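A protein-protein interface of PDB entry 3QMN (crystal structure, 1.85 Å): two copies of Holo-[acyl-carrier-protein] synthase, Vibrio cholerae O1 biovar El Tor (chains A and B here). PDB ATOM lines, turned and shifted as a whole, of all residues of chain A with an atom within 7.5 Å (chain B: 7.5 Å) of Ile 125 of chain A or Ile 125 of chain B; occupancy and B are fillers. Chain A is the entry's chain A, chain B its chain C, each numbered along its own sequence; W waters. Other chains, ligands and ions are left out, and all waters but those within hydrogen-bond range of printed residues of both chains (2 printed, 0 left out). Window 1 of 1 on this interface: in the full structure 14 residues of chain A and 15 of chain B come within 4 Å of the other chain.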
ATOM      1  N   MET A   4     -15.418  24.091  30.492  1.00  0.00           N
ATOM      2  CA  MET A   4     -16.532  24.672  29.820  1.00  0.00           C
ATOM      3  C   MET A   4     -16.042  25.775  28.899  1.00  0.00           C
ATOM      4  O   MET A   4     -14.924  26.298  29.022  1.00  0.00           O
ATOM      5  CB  MET A   4     -17.573  25.265  30.777  1.00  0.00           C
ATOM      6  CG  MET A   4     -17.217  26.577  31.412  1.00  0.00           C
ATOM      7  SD  MET A   4     -18.681  27.168  32.566  1.00  0.00           S
ATOM      8  CE  MET A   4     -18.627  25.725  33.887  1.00  0.00           C
ATOM      9  N   ILE A   5     -16.923  26.119  27.985  1.00  0.00           N
ATOM     10  CA  ILE A   5     -16.666  27.146  27.017  1.00  0.00           C
ATOM     11  C   ILE A   5     -16.832  28.492  27.680  1.00  0.00           C
ATOM     12  O   ILE A   5     -17.852  28.750  28.332  1.00  0.00           O
ATOM     13  CB  ILE A   5     -17.670  27.024  25.871  1.00  0.00           C
ATOM     14  CG1 ILE A   5     -17.396  25.741  25.095  1.00  0.00           C
ATOM     15  CG2 ILE A   5     -17.524  28.208  24.921  1.00  0.00           C
ATOM     16  CD1 ILE A   5     -18.493  25.365  24.093  1.00  0.00           C
ATOM     17  N   VAL A   6     -15.832  29.346  27.541  1.00  0.00           N
ATOM     18  CA  VAL A   6     -15.907  30.665  28.134  1.00  0.00           C
ATOM     19  C   VAL A   6     -16.089  31.766  27.093  1.00  0.00           C
ATOM     20  O   VAL A   6     -16.352  32.915  27.444  1.00  0.00           O
ATOM     21  CB  VAL A   6     -14.726  30.924  29.129  1.00  0.00           C
ATOM     22  CG1 VAL A   6     -14.865  30.022  30.333  1.00  0.00           C
ATOM     23  CG2 VAL A   6     -13.387  30.735  28.452  1.00  0.00           C
ATOM     24  N   GLY A   7     -15.991  31.425  25.811  1.00  0.00           N
ATOM     25  CA  GLY A   7     -16.172  32.427  24.761  1.00  0.00           C
ATOM     26  C   GLY A   7     -16.270  31.810  23.386  1.00  0.00           C
ATOM     27  O   GLY A   7     -15.658  30.779  23.104  1.00  0.00           O
ATOM     28  N   LEU A   8     -17.072  32.449  22.543  1.00  0.00           N
ATOM     29  CA  LEU A   8     -17.313  32.035  21.170  1.00  0.00           C
ATOM     30  C   LEU A   8     -17.292  33.276  20.311  1.00  0.00           C
ATOM     31  O   LEU A   8     -17.929  34.271  20.657  1.00  0.00           O
ATOM     32  CB  LEU A   8     -18.686  31.413  21.040  1.00  0.00           C
ATOM     33  CG  LEU A   8     -19.161  31.093  19.620  1.00  0.00           C
ATOM     34  CD1 LEU A   8     -18.266  30.085  18.892  1.00  0.00           C
ATOM     35  CD2 LEU A   8     -20.606  30.575  19.691  1.00  0.00           C
ATOM     36  N   GLY A   9     -16.577  33.207  19.194  1.00  0.00           N
ATOM     37  CA  GLY A   9     -16.489  34.331  18.266  1.00  0.00           C
ATOM     38  C   GLY A   9     -16.473  33.875  16.827  1.00  0.00           C
ATOM     39  O   GLY A   9     -15.922  32.837  16.510  1.00  0.00           O
ATOM     40  N   ALA A  61     -12.704  37.469  15.197  1.00  0.00           N
ATOM     41  CA  ALA A  61     -13.421  36.338  15.839  1.00  0.00           C
ATOM     42  C   ALA A  61     -12.858  36.119  17.263  1.00  0.00           C
ATOM     43  O   ALA A  61     -13.607  35.903  18.236  1.00  0.00           O
ATOM     44  CB  ALA A  61     -13.274  35.030  14.992  1.00  0.00           C
ATOM     45  N   ALA A  62     -11.536  36.122  17.392  1.00  0.00           N
ATOM     46  CA  ALA A  62     -10.926  35.916  18.713  1.00  0.00           C
ATOM     47  C   ALA A  62     -11.319  37.023  19.700  1.00  0.00           C
ATOM     48  O   ALA A  62     -11.549  36.765  20.884  1.00  0.00           O
ATOM     49  CB  ALA A  62      -9.421  35.839  18.584  1.00  0.00           C
ATOM     50  N   ALA A  65     -14.687  36.319  20.996  1.00  0.00           N
ATOM     51  CA  ALA A  65     -14.687  35.199  21.913  1.00  0.00           C
ATOM     52  C   ALA A  65     -14.248  35.680  23.309  1.00  0.00           C
ATOM     53  O   ALA A  65     -14.709  35.176  24.310  1.00  0.00           O
ATOM     54  CB  ALA A  65     -13.787  34.071  21.380  1.00  0.00           C
ATOM     55  N   LEU A  91      -3.695  29.963  17.788  1.00  0.00           N
ATOM     56  CA  LEU A  91      -3.835  31.333  18.289  1.00  0.00           C
ATOM     57  C   LEU A  91      -3.155  31.485  19.646  1.00  0.00           C
ATOM     58  O   LEU A  91      -3.398  30.707  20.570  1.00  0.00           O
ATOM     59  CB  LEU A  91      -5.329  31.673  18.390  1.00  0.00           C
ATOM     60  CG  LEU A  91      -5.777  32.999  18.983  1.00  0.00           C
ATOM     61  CD1 LEU A  91      -5.157  34.189  18.238  1.00  0.00           C
ATOM     62  CD2 LEU A  91      -7.306  33.073  18.981  1.00  0.00           C
ATOM     63  N   VAL A 106      -8.923  30.809  30.778  1.00  0.00           N
ATOM     64  CA  VAL A 106      -8.778  30.134  29.487  1.00  0.00           C
ATOM     65  C   VAL A 106      -7.542  29.225  29.498  1.00  0.00           C
ATOM     66  O   VAL A 106      -6.428  29.660  29.795  1.00  0.00           O
ATOM     67  CB  VAL A 106      -8.689  31.129  28.332  1.00  0.00           C
ATOM     68  CG1 VAL A 106      -8.384  30.413  26.973  1.00  0.00           C
ATOM     69  CG2 VAL A 106     -10.001  31.970  28.239  1.00  0.00           C
ATOM     70  N   ASN A 108      -7.506  26.480  26.891  1.00  0.00           N
ATOM     71  CA  ASN A 108      -7.419  25.954  25.541  1.00  0.00           C
ATOM     72  C   ASN A 108      -8.132  26.903  24.580  1.00  0.00           C
ATOM     73  O   ASN A 108      -9.210  27.417  24.888  1.00  0.00           O
ATOM     74  CB  ASN A 108      -8.037  24.568  25.498  1.00  0.00           C
ATOM     75  CG  ASN A 108      -7.220  23.539  26.255  1.00  0.00           C
ATOM     76  OD1 ASN A 108      -6.022  23.402  26.025  1.00  0.00           O
ATOM     77  ND2 ASN A 108      -7.872  22.786  27.127  1.00  0.00           N
ATOM     78  N   ILE A 109      -7.492  27.146  23.440  1.00  0.00           N
ATOM     79  CA  ILE A 109      -8.011  28.037  22.428  1.00  0.00           C
ATOM     80  C   ILE A 109      -8.115  27.279  21.118  1.00  0.00           C
ATOM     81  O   ILE A 109      -7.137  26.651  20.691  1.00  0.00           O
ATOM     82  CB  ILE A 109      -7.038  29.211  22.212  1.00  0.00           C
ATOM     83  CG1 ILE A 109      -6.783  29.947  23.531  1.00  0.00           C
ATOM     84  CG2 ILE A 109      -7.566  30.164  21.133  1.00  0.00           C
ATOM     85  CD1 ILE A 109      -5.650  30.937  23.448  1.00  0.00           C
ATOM     86  N   HIS A 110      -9.274  27.354  20.475  1.00  0.00           N
ATOM     87  CA  HIS A 110      -9.484  26.687  19.216  1.00  0.00           C
ATOM     88  C   HIS A 110      -9.857  27.753  18.183  1.00  0.00           C
ATOM     89  O   HIS A 110     -10.667  28.630  18.457  1.00  0.00           O
ATOM     90  CB  HIS A 110     -10.593  25.660  19.330  1.00  0.00           C
ATOM     91  CG  HIS A 110     -10.370  24.687  20.440  1.00  0.00           C
ATOM     92  ND1 HIS A 110      -9.597  23.562  20.288  1.00  0.00           N
ATOM     93  CD2 HIS A 110     -10.736  24.723  21.741  1.00  0.00           C
ATOM     94  CE1 HIS A 110      -9.520  22.926  21.441  1.00  0.00           C
ATOM     95  NE2 HIS A 110     -10.207  23.607  22.339  1.00  0.00           N
ATOM     96  N   LEU A 111      -9.300  27.608  16.995  1.00  0.00           N
ATOM     97  CA  LEU A 111      -9.505  28.502  15.863  1.00  0.00           C
ATOM     98  C   LEU A 111      -9.588  27.710  14.583  1.00  0.00           C
ATOM     99  O   LEU A 111      -8.835  26.746  14.394  1.00  0.00           O
ATOM    100  CB  LEU A 111      -8.285  29.432  15.725  1.00  0.00           C
ATOM    101  CG  LEU A 111      -8.059  30.279  14.460  1.00  0.00           C
ATOM    102  CD1 LEU A 111      -9.232  31.261  14.164  1.00  0.00           C
ATOM    103  CD2 LEU A 111      -6.734  31.053  14.552  1.00  0.00           C
ATOM    104  N   SER A 112     -10.536  28.075  13.726  1.00  0.00           N
ATOM    105  CA  SER A 112     -10.633  27.495  12.385  1.00  0.00           C
ATOM    106  C   SER A 112     -10.871  28.657  11.450  1.00  0.00           C
ATOM    107  O   SER A 112     -11.566  29.605  11.822  1.00  0.00           O
ATOM    108  CB  SER A 112     -11.753  26.497  12.213  1.00  0.00           C
ATOM    109  OG  SER A 112     -11.619  25.865  10.955  1.00  0.00           O
ATOM    110  N   THR A 123     -13.799  31.115  13.075  1.00  0.00           N
ATOM    111  CA  THR A 123     -14.476  30.860  14.333  1.00  0.00           C
ATOM    112  C   THR A 123     -13.443  30.521  15.389  1.00  0.00           C
ATOM    113  O   THR A 123     -12.446  29.835  15.125  1.00  0.00           O
ATOM    114  CB  THR A 123     -15.543  29.751  14.229  1.00  0.00           C
ATOM    115  OG1 THR A 123     -16.571  30.201  13.327  1.00  0.00           O
ATOM    116  CG2 THR A 123     -16.170  29.442  15.620  1.00  0.00           C
ATOM    117  N   VAL A 124     -13.661  31.043  16.587  1.00  0.00           N
ATOM    118  CA  VAL A 124     -12.789  30.816  17.729  1.00  0.00           C
ATOM    119  C   VAL A 124     -13.591  30.406  18.951  1.00  0.00           C
ATOM    120  O   VAL A 124     -14.652  30.968  19.225  1.00  0.00           O
ATOM    121  CB  VAL A 124     -12.001  32.103  18.086  1.00  0.00           C
ATOM    122  CG1 VAL A 124     -11.229  31.958  19.467  1.00  0.00           C
ATOM    123  CG2 VAL A 124     -11.049  32.465  16.964  1.00  0.00           C
ATOM    124  N   ILE A 125     -13.109  29.387  19.654  1.00  0.00           N
ATOM    125  CA  ILE A 125     -13.732  28.948  20.897  1.00  0.00           C
ATOM    126  C   ILE A 125     -12.665  28.965  21.993  1.00  0.00           C
ATOM    127  O   ILE A 125     -11.568  28.439  21.800  1.00  0.00           O
ATOM    128  CB  ILE A 125     -14.292  27.522  20.833  1.00  0.00           C
ATOM    129  CG1 ILE A 125     -15.431  27.442  19.831  1.00  0.00           C
ATOM    130  CG2 ILE A 125     -14.819  27.102  22.196  1.00  0.00           C
ATOM    131  CD1 ILE A 125     -15.907  26.029  19.514  1.00  0.00           C
ATOM    132  N   LEU A 126     -12.989  29.571  23.119  1.00  0.00           N
ATOM    133  CA  LEU A 126     -12.063  29.612  24.254  1.00  0.00           C
ATOM    134  C   LEU A 126     -12.654  28.698  25.307  1.00  0.00           C
ATOM    135  O   LEU A 126     -13.861  28.755  25.570  1.00  0.00           O
ATOM    136  CB  LEU A 126     -11.932  31.001  24.819  1.00  0.00           C
ATOM    137  CG  LEU A 126     -11.549  32.133  23.883  1.00  0.00           C
ATOM    138  CD1 LEU A 126     -11.596  33.462  24.646  1.00  0.00           C
ATOM    139  CD2 LEU A 126     -10.182  31.871  23.257  1.00  0.00           C
ATOM    140  N   GLU A 127     -11.837  27.841  25.907  1.00  0.00           N
ATOM    141  CA  GLU A 127     -12.356  26.944  26.945  1.00  0.00           C
ATOM    142  C   GLU A 127     -11.482  26.933  28.189  1.00  0.00           C
ATOM    143  O   GLU A 127     -10.286  27.165  28.123  1.00  0.00           O
ATOM    144  CB  GLU A 127     -12.560  25.497  26.472  1.00  0.00           C
ATOM    145  CG  GLU A 127     -11.338  24.795  25.957  1.00  0.00           C
ATOM    146  CD  GLU A 127     -11.584  23.322  25.567  1.00  0.00           C
ATOM    147  OE1 GLU A 127     -10.902  22.851  24.632  1.00  0.00           O
ATOM    148  OE2 GLU A 127     -12.443  22.640  26.180  1.00  0.00           O
ATOM    149  N   MET B   4     -13.465  17.940  26.994  1.00  0.00           N
ATOM    150  CA  MET B   4     -12.946  19.123  26.358  1.00  0.00           C
ATOM    151  C   MET B   4     -13.028  19.005  24.841  1.00  0.00           C
ATOM    152  O   MET B   4     -13.306  17.949  24.277  1.00  0.00           O
ATOM    153  CB  MET B   4     -11.504  19.397  26.784  1.00  0.00           C
ATOM    154  CG  MET B   4     -10.470  18.482  26.208  1.00  0.00           C
ATOM    155  SD  MET B   4      -8.741  18.885  26.991  1.00  0.00           S
ATOM    156  CE  MET B   4      -9.122  18.244  28.792  1.00  0.00           C
ATOM    157  N   ILE B   5     -12.811  20.132  24.193  1.00  0.00           N
ATOM    158  CA  ILE B   5     -12.855  20.198  22.747  1.00  0.00           C
ATOM    159  C   ILE B   5     -11.532  19.732  22.176  1.00  0.00           C
ATOM    160  O   ILE B   5     -10.467  20.245  22.555  1.00  0.00           O
ATOM    161  CB  ILE B   5     -13.156  21.615  22.287  1.00  0.00           C
ATOM    162  CG1 ILE B   5     -14.578  21.998  22.700  1.00  0.00           C
ATOM    163  CG2 ILE B   5     -13.015  21.721  20.763  1.00  0.00           C
ATOM    164  CD1 ILE B   5     -14.895  23.498  22.485  1.00  0.00           C
ATOM    165  N   VAL B   6     -11.625  18.781  21.267  1.00  0.00           N
ATOM    166  CA  VAL B   6     -10.482  18.163  20.589  1.00  0.00           C
ATOM    167  C   VAL B   6     -10.137  18.950  19.327  1.00  0.00           C
ATOM    168  O   VAL B   6      -8.966  19.112  18.959  1.00  0.00           O
ATOM    169  CB  VAL B   6     -10.858  16.695  20.195  1.00  0.00           C
ATOM    170  CG1 VAL B   6      -9.847  16.063  19.212  1.00  0.00           C
ATOM    171  CG2 VAL B   6     -11.027  15.862  21.415  1.00  0.00           C
ATOM    172  N   GLY B   7     -11.173  19.461  18.684  1.00  0.00           N
ATOM    173  CA  GLY B   7     -10.987  20.233  17.461  1.00  0.00           C
ATOM    174  C   GLY B   7     -12.185  20.999  17.010  1.00  0.00           C
ATOM    175  O   GLY B   7     -13.324  20.726  17.406  1.00  0.00           O
ATOM    176  N   LEU B   8     -11.910  21.996  16.172  1.00  0.00           N
ATOM    177  CA  LEU B   8     -12.907  22.859  15.601  1.00  0.00           C
ATOM    178  C   LEU B   8     -12.571  23.079  14.148  1.00  0.00           C
ATOM    179  O   LEU B   8     -11.398  23.296  13.813  1.00  0.00           O
ATOM    180  CB  LEU B   8     -12.827  24.207  16.301  1.00  0.00           C
ATOM    181  CG  LEU B   8     -13.609  25.366  15.745  1.00  0.00           C
ATOM    182  CD1 LEU B   8     -15.155  25.174  15.774  1.00  0.00           C
ATOM    183  CD2 LEU B   8     -13.214  26.695  16.474  1.00  0.00           C
ATOM    184  N   GLY B   9     -13.572  22.961  13.295  1.00  0.00           N
ATOM    185  CA  GLY B   9     -13.390  23.195  11.880  1.00  0.00           C
ATOM    186  C   GLY B   9     -14.549  23.977  11.294  1.00  0.00           C
ATOM    187  O   GLY B   9     -15.691  23.860  11.744  1.00  0.00           O
ATOM    188  N   ALA B  61     -14.876  20.955   6.785  1.00  0.00           N
ATOM    189  CA  ALA B  61     -14.902  21.432   8.165  1.00  0.00           C
ATOM    190  C   ALA B  61     -14.505  20.291   9.122  1.00  0.00           C
ATOM    191  O   ALA B  61     -13.714  20.500  10.043  1.00  0.00           O
ATOM    192  CB  ALA B  61     -16.321  21.992   8.539  1.00  0.00           C
ATOM    193  N   ALA B  62     -15.031  19.098   8.886  1.00  0.00           N
ATOM    194  CA  ALA B  62     -14.733  17.943   9.731  1.00  0.00           C
ATOM    195  C   ALA B  62     -13.242  17.635   9.698  1.00  0.00           C
ATOM    196  O   ALA B  62     -12.648  17.349  10.730  1.00  0.00           O
ATOM    197  CB  ALA B  62     -15.556  16.705   9.285  1.00  0.00           C
ATOM    198  N   ALA B  65     -11.372  20.003  11.889  1.00  0.00           N
ATOM    199  CA  ALA B  65     -11.609  19.692  13.306  1.00  0.00           C
ATOM    200  C   ALA B  65     -10.699  18.547  13.759  1.00  0.00           C
ATOM    201  O   ALA B  65     -10.256  18.513  14.911  1.00  0.00           O
ATOM    202  CB  ALA B  65     -13.104  19.344  13.572  1.00  0.00           C
ATOM    203  N   LEU B  91     -22.536  13.512  11.785  1.00  0.00           N
ATOM    204  CA  LEU B  91     -21.265  13.178  11.154  1.00  0.00           C
ATOM    205  C   LEU B  91     -20.691  11.914  11.773  1.00  0.00           C
ATOM    206  O   LEU B  91     -20.549  11.835  12.998  1.00  0.00           O
ATOM    207  CB  LEU B  91     -20.291  14.314  11.427  1.00  0.00           C
ATOM    208  CG  LEU B  91     -18.832  14.161  11.007  1.00  0.00           C
ATOM    209  CD1 LEU B  91     -18.748  13.922   9.516  1.00  0.00           C
ATOM    210  CD2 LEU B  91     -18.055  15.432  11.418  1.00  0.00           C
ATOM    211  N   VAL B 106     -12.017  11.029  20.929  1.00  0.00           N
ATOM    212  CA  VAL B 106     -13.234  11.733  20.536  1.00  0.00           C
ATOM    213  C   VAL B 106     -14.431  10.875  20.898  1.00  0.00           C
ATOM    214  O   VAL B 106     -14.461   9.679  20.565  1.00  0.00           O
ATOM    215  CB  VAL B 106     -13.277  12.032  19.038  1.00  0.00           C
ATOM    216  CG1 VAL B 106     -14.696  12.534  18.599  1.00  0.00           C
ATOM    217  CG2 VAL B 106     -12.173  13.034  18.680  1.00  0.00           C
ATOM    218  N   ASN B 108     -17.808  12.631  21.159  1.00  0.00           N
ATOM    219  CA  ASN B 108     -18.981  13.325  20.687  1.00  0.00           C
ATOM    220  C   ASN B 108     -18.607  14.219  19.527  1.00  0.00           C
ATOM    221  O   ASN B 108     -17.589  14.906  19.551  1.00  0.00           O
ATOM    222  CB  ASN B 108     -19.633  14.063  21.836  1.00  0.00           C
ATOM    223  CG  ASN B 108     -20.325  13.096  22.794  1.00  0.00           C
ATOM    224  OD1 ASN B 108     -21.308  12.435  22.426  1.00  0.00           O
ATOM    225  ND2 ASN B 108     -19.822  13.002  24.000  1.00  0.00           N
ATOM    226  N   ILE B 109     -19.436  14.161  18.507  1.00  0.00           N
ATOM    227  CA  ILE B 109     -19.214  14.907  17.299  1.00  0.00           C
ATOM    228  C   ILE B 109     -20.410  15.783  16.991  1.00  0.00           C
ATOM    229  O   ILE B 109     -21.529  15.293  16.995  1.00  0.00           O
ATOM    230  CB  ILE B 109     -18.994  13.906  16.161  1.00  0.00           C
ATOM    231  CG1 ILE B 109     -17.738  13.055  16.474  1.00  0.00           C
ATOM    232  CG2 ILE B 109     -18.859  14.612  14.832  1.00  0.00           C
ATOM    233  CD1 ILE B 109     -17.375  12.049  15.355  1.00  0.00           C
ATOM    234  N   HIS B 110     -20.169  17.059  16.678  1.00  0.00           N
ATOM    235  CA  HIS B 110     -21.239  17.984  16.363  1.00  0.00           C
ATOM    236  C   HIS B 110     -20.975  18.687  15.036  1.00  0.00           C
ATOM    237  O   HIS B 110     -19.870  19.128  14.757  1.00  0.00           O
ATOM    238  CB  HIS B 110     -21.379  19.036  17.454  1.00  0.00           C
ATOM    239  CG  HIS B 110     -21.517  18.451  18.817  1.00  0.00           C
ATOM    240  ND1 HIS B 110     -22.728  18.067  19.334  1.00  0.00           N
ATOM    241  CD2 HIS B 110     -20.585  18.135  19.744  1.00  0.00           C
ATOM    242  CE1 HIS B 110     -22.543  17.549  20.533  1.00  0.00           C
ATOM    243  NE2 HIS B 110     -21.253  17.596  20.810  1.00  0.00           N
ATOM    244  N   LEU B 111     -22.018  18.769  14.240  1.00  0.00           N
ATOM    245  CA  LEU B 111     -21.989  19.385  12.925  1.00  0.00           C
ATOM    246  C   LEU B 111     -23.229  20.242  12.691  1.00  0.00           C
ATOM    247  O   LEU B 111     -24.318  19.861  13.124  1.00  0.00           O
ATOM    248  CB  LEU B 111     -22.049  18.264  11.884  1.00  0.00           C
ATOM    249  CG  LEU B 111     -22.311  18.568  10.384  1.00  0.00           C
ATOM    250  CD1 LEU B 111     -21.205  19.446   9.697  1.00  0.00           C
ATOM    251  CD2 LEU B 111     -22.469  17.274   9.600  1.00  0.00           C
ATOM    252  N   SER B 112     -23.065  21.397  12.050  1.00  0.00           N
ATOM    253  CA  SER B 112     -24.210  22.221  11.641  1.00  0.00           C
ATOM    254  C   SER B 112     -23.846  22.700  10.231  1.00  0.00           C
ATOM    255  O   SER B 112     -22.670  22.978   9.941  1.00  0.00           O
ATOM    256  CB  SER B 112     -24.482  23.432  12.534  1.00  0.00           C
ATOM    257  OG  SER B 112     -25.710  24.075  12.140  1.00  0.00           O
ATOM    258  N   THR B 123     -19.813  23.987  10.215  1.00  0.00           N
ATOM    259  CA  THR B 123     -18.933  24.030  11.362  1.00  0.00           C
ATOM    260  C   THR B 123     -19.045  22.669  12.057  1.00  0.00           C
ATOM    261  O   THR B 123     -20.121  22.098  12.123  1.00  0.00           O
ATOM    262  CB  THR B 123     -19.239  25.166  12.330  1.00  0.00           C
ATOM    263  OG1 THR B 123     -18.968  26.429  11.687  1.00  0.00           O
ATOM    264  CG2 THR B 123     -18.329  25.071  13.572  1.00  0.00           C
ATOM    265  N   VAL B 124     -17.911  22.193  12.565  1.00  0.00           N
ATOM    266  CA  VAL B 124     -17.792  20.910  13.249  1.00  0.00           C
ATOM    267  C   VAL B 124     -16.966  21.084  14.505  1.00  0.00           C
ATOM    268  O   VAL B 124     -15.995  21.847  14.533  1.00  0.00           O
ATOM    269  CB  VAL B 124     -17.077  19.827  12.377  1.00  0.00           C
ATOM    270  CG1 VAL B 124     -16.840  18.571  13.212  1.00  0.00           C
ATOM    271  CG2 VAL B 124     -17.893  19.467  11.078  1.00  0.00           C
ATOM    272  N   ILE B 125     -17.399  20.403  15.567  1.00  0.00           N
ATOM    273  CA  ILE B 125     -16.671  20.393  16.810  1.00  0.00           C
ATOM    274  C   ILE B 125     -16.580  18.933  17.256  1.00  0.00           C
ATOM    275  O   ILE B 125     -17.586  18.197  17.218  1.00  0.00           O
ATOM    276  CB  ILE B 125     -17.353  21.220  17.946  1.00  0.00           C
ATOM    277  CG1 ILE B 125     -17.537  22.689  17.545  1.00  0.00           C
ATOM    278  CG2 ILE B 125     -16.544  21.063  19.315  1.00  0.00           C
ATOM    279  CD1 ILE B 125     -18.425  23.477  18.547  1.00  0.00           C
ATOM    280  N   LEU B 126     -15.365  18.530  17.645  1.00  0.00           N
ATOM    281  CA  LEU B 126     -15.076  17.200  18.161  1.00  0.00           C
ATOM    282  C   LEU B 126     -14.788  17.394  19.646  1.00  0.00           C
ATOM    283  O   LEU B 126     -13.967  18.236  20.035  1.00  0.00           O
ATOM    284  CB  LEU B 126     -13.874  16.557  17.456  1.00  0.00           C
ATOM    285  CG  LEU B 126     -13.930  16.489  15.924  1.00  0.00           C
ATOM    286  CD1 LEU B 126     -12.660  15.828  15.396  1.00  0.00           C
ATOM    287  CD2 LEU B 126     -15.203  15.747  15.393  1.00  0.00           C
ATOM    288  N   GLU B 127     -15.412  16.552  20.468  1.00  0.00           N
ATOM    289  CA  GLU B 127     -15.306  16.647  21.918  1.00  0.00           C
ATOM    290  C   GLU B 127     -14.915  15.304  22.519  1.00  0.00           C
ATOM    291  O   GLU B 127     -15.333  14.259  22.008  1.00  0.00           O
ATOM    292  CB  GLU B 127     -16.696  17.058  22.399  1.00  0.00           C
ATOM    293  CG  GLU B 127     -16.948  17.044  23.835  1.00  0.00           C
ATOM    294  CD  GLU B 127     -18.446  17.120  24.174  1.00  0.00           C
ATOM    295  OE1 GLU B 127     -19.279  17.499  23.311  1.00  0.00           O
ATOM    296  OE2 GLU B 127     -18.778  16.752  25.312  1.00  0.00           O
HETATM  297  O   HOH W   1     -18.917  28.698  13.318  1.00  0.00           O
HETATM  298  O   HOH W   2      -8.832  24.117  13.379  1.00  0.00           O
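Among the printed residues, pairs that only touch across the chains: Ser 112 of chain A with Gly 9 of chain B (3.3 Å), Glu 127 of chain A with Met 4 of chain B (3.4 Å), Thr 123 of chain A with Leu 8 of chain B (3.5 Å), Ser 112 of chain A with Leu 8 of chain B (3.6 Å), Ile 125 of chain A with Ile 5 of chain B (3.6 Å), Ile 125 of chain A with Ile 125 of chain B (3.7 Å), His 110 of chain A with Leu 8 of chain B (3.8 Å), Ile 125 of chain A with Leu 8 of chain B (3.9 Å) and Asn 108 of chain A with Met 4 of chain B (3.999 Å).
Of chain B, only Ile 5, Leu 8 and Ile 125 come within 4 Å of Ile 125 of chain A.
Ile 125 of chain B touches one residue of chain A.
Of the printed residues of chain A, Gly 9 of chain B touches Ser 112.
Printed residues of chain B within 4 Å of Ser 112 of chain A: Leu 8 (3.6 Å) and Gly 9 (3.3 Å).
Val 6 of chain B touches none of the printed residues of chain A.
The nearest residue of chain A that does not touch Ile 125 of chain B is Ile 5 of chain A (5.9 Å).
Of the 21 printed residues of chain A, 6 touch a printed residue of chain B.
Printed residues of chain A that touch a printed residue of chain B: Asn 108, His 110, Ser 112, Thr 123, Ile 125 and Glu 127.
Hydrophobic or aromatic side chains of chain A that line the printed part of chain B: His 110 and Ile 125.
Along chain A the printed residues that touch a printed residue of chain B span positions 108 to 127.
OE2 of Glu 127 of chain A lies within hydrogen-bond range of N of Ile 5 of chain B, at 3.2 Å.
A ring nitrogen (NE2) of His 110 of chain A lies close to the backbone carbonyl oxygen (O) of Ile 5 of chain B (3.4 Å).
His 110 of chain A touches Leu 8 of chain B, but with the chains exchanged Leu 8 of chain A does not touch His 110 of chain B (11.6 Å).
Ser 112 of chain A touches Gly 9 of chain B, but with the chains exchanged Gly 9 of chain A does not touch Ser 112 of chain B (13.3 Å).
Thr 123 of chain A touches Leu 8 of chain B, but with the chains exchanged Leu 8 of chain A does not touch Thr 123 of chain B (7.3 Å).
Ile 125 of chain A touches Leu 8 of chain B, but with the chains exchanged Leu 8 of chain A does not touch Ile 125 of chain B (6.6 Å).
O of Thr 123 of chain A is in hydrogen-bond range of N of Ser 112 of chain A (3.0 Å).
A ring nitrogen (NE2) of His 110 of chain A is in hydrogen-bond range of the side-chain carboxylate (OE1) of Glu 127 of chain A (2.5 Å).
The backbone carbonyl oxygen of Gly 9 of chain B sits at hydrogen-bond distance from the backbone NH of Val 124 of chain B (2.9 Å).
O of Ile 125 of chain B is in hydrogen-bond range of N of His 110 of chain B, at 2.9 Å.
N of Glu 127 of chain A lies within hydrogen-bond range of O of Asn 108 of chain A.
The backbone carbonyl oxygen of His 110 of chain A lies within hydrogen-bond range of the backbone NH of Ile 125 of chain A.
Water W2 bridges O of Leu 8 of chain B (2.7 Å) and O of Leu 111 of chain A (2.8 Å).
Water W1 bridges OG1 of Thr 123 of chain A (2.8 Å) and OG1 of Thr 123 of chain B (2.8 Å).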
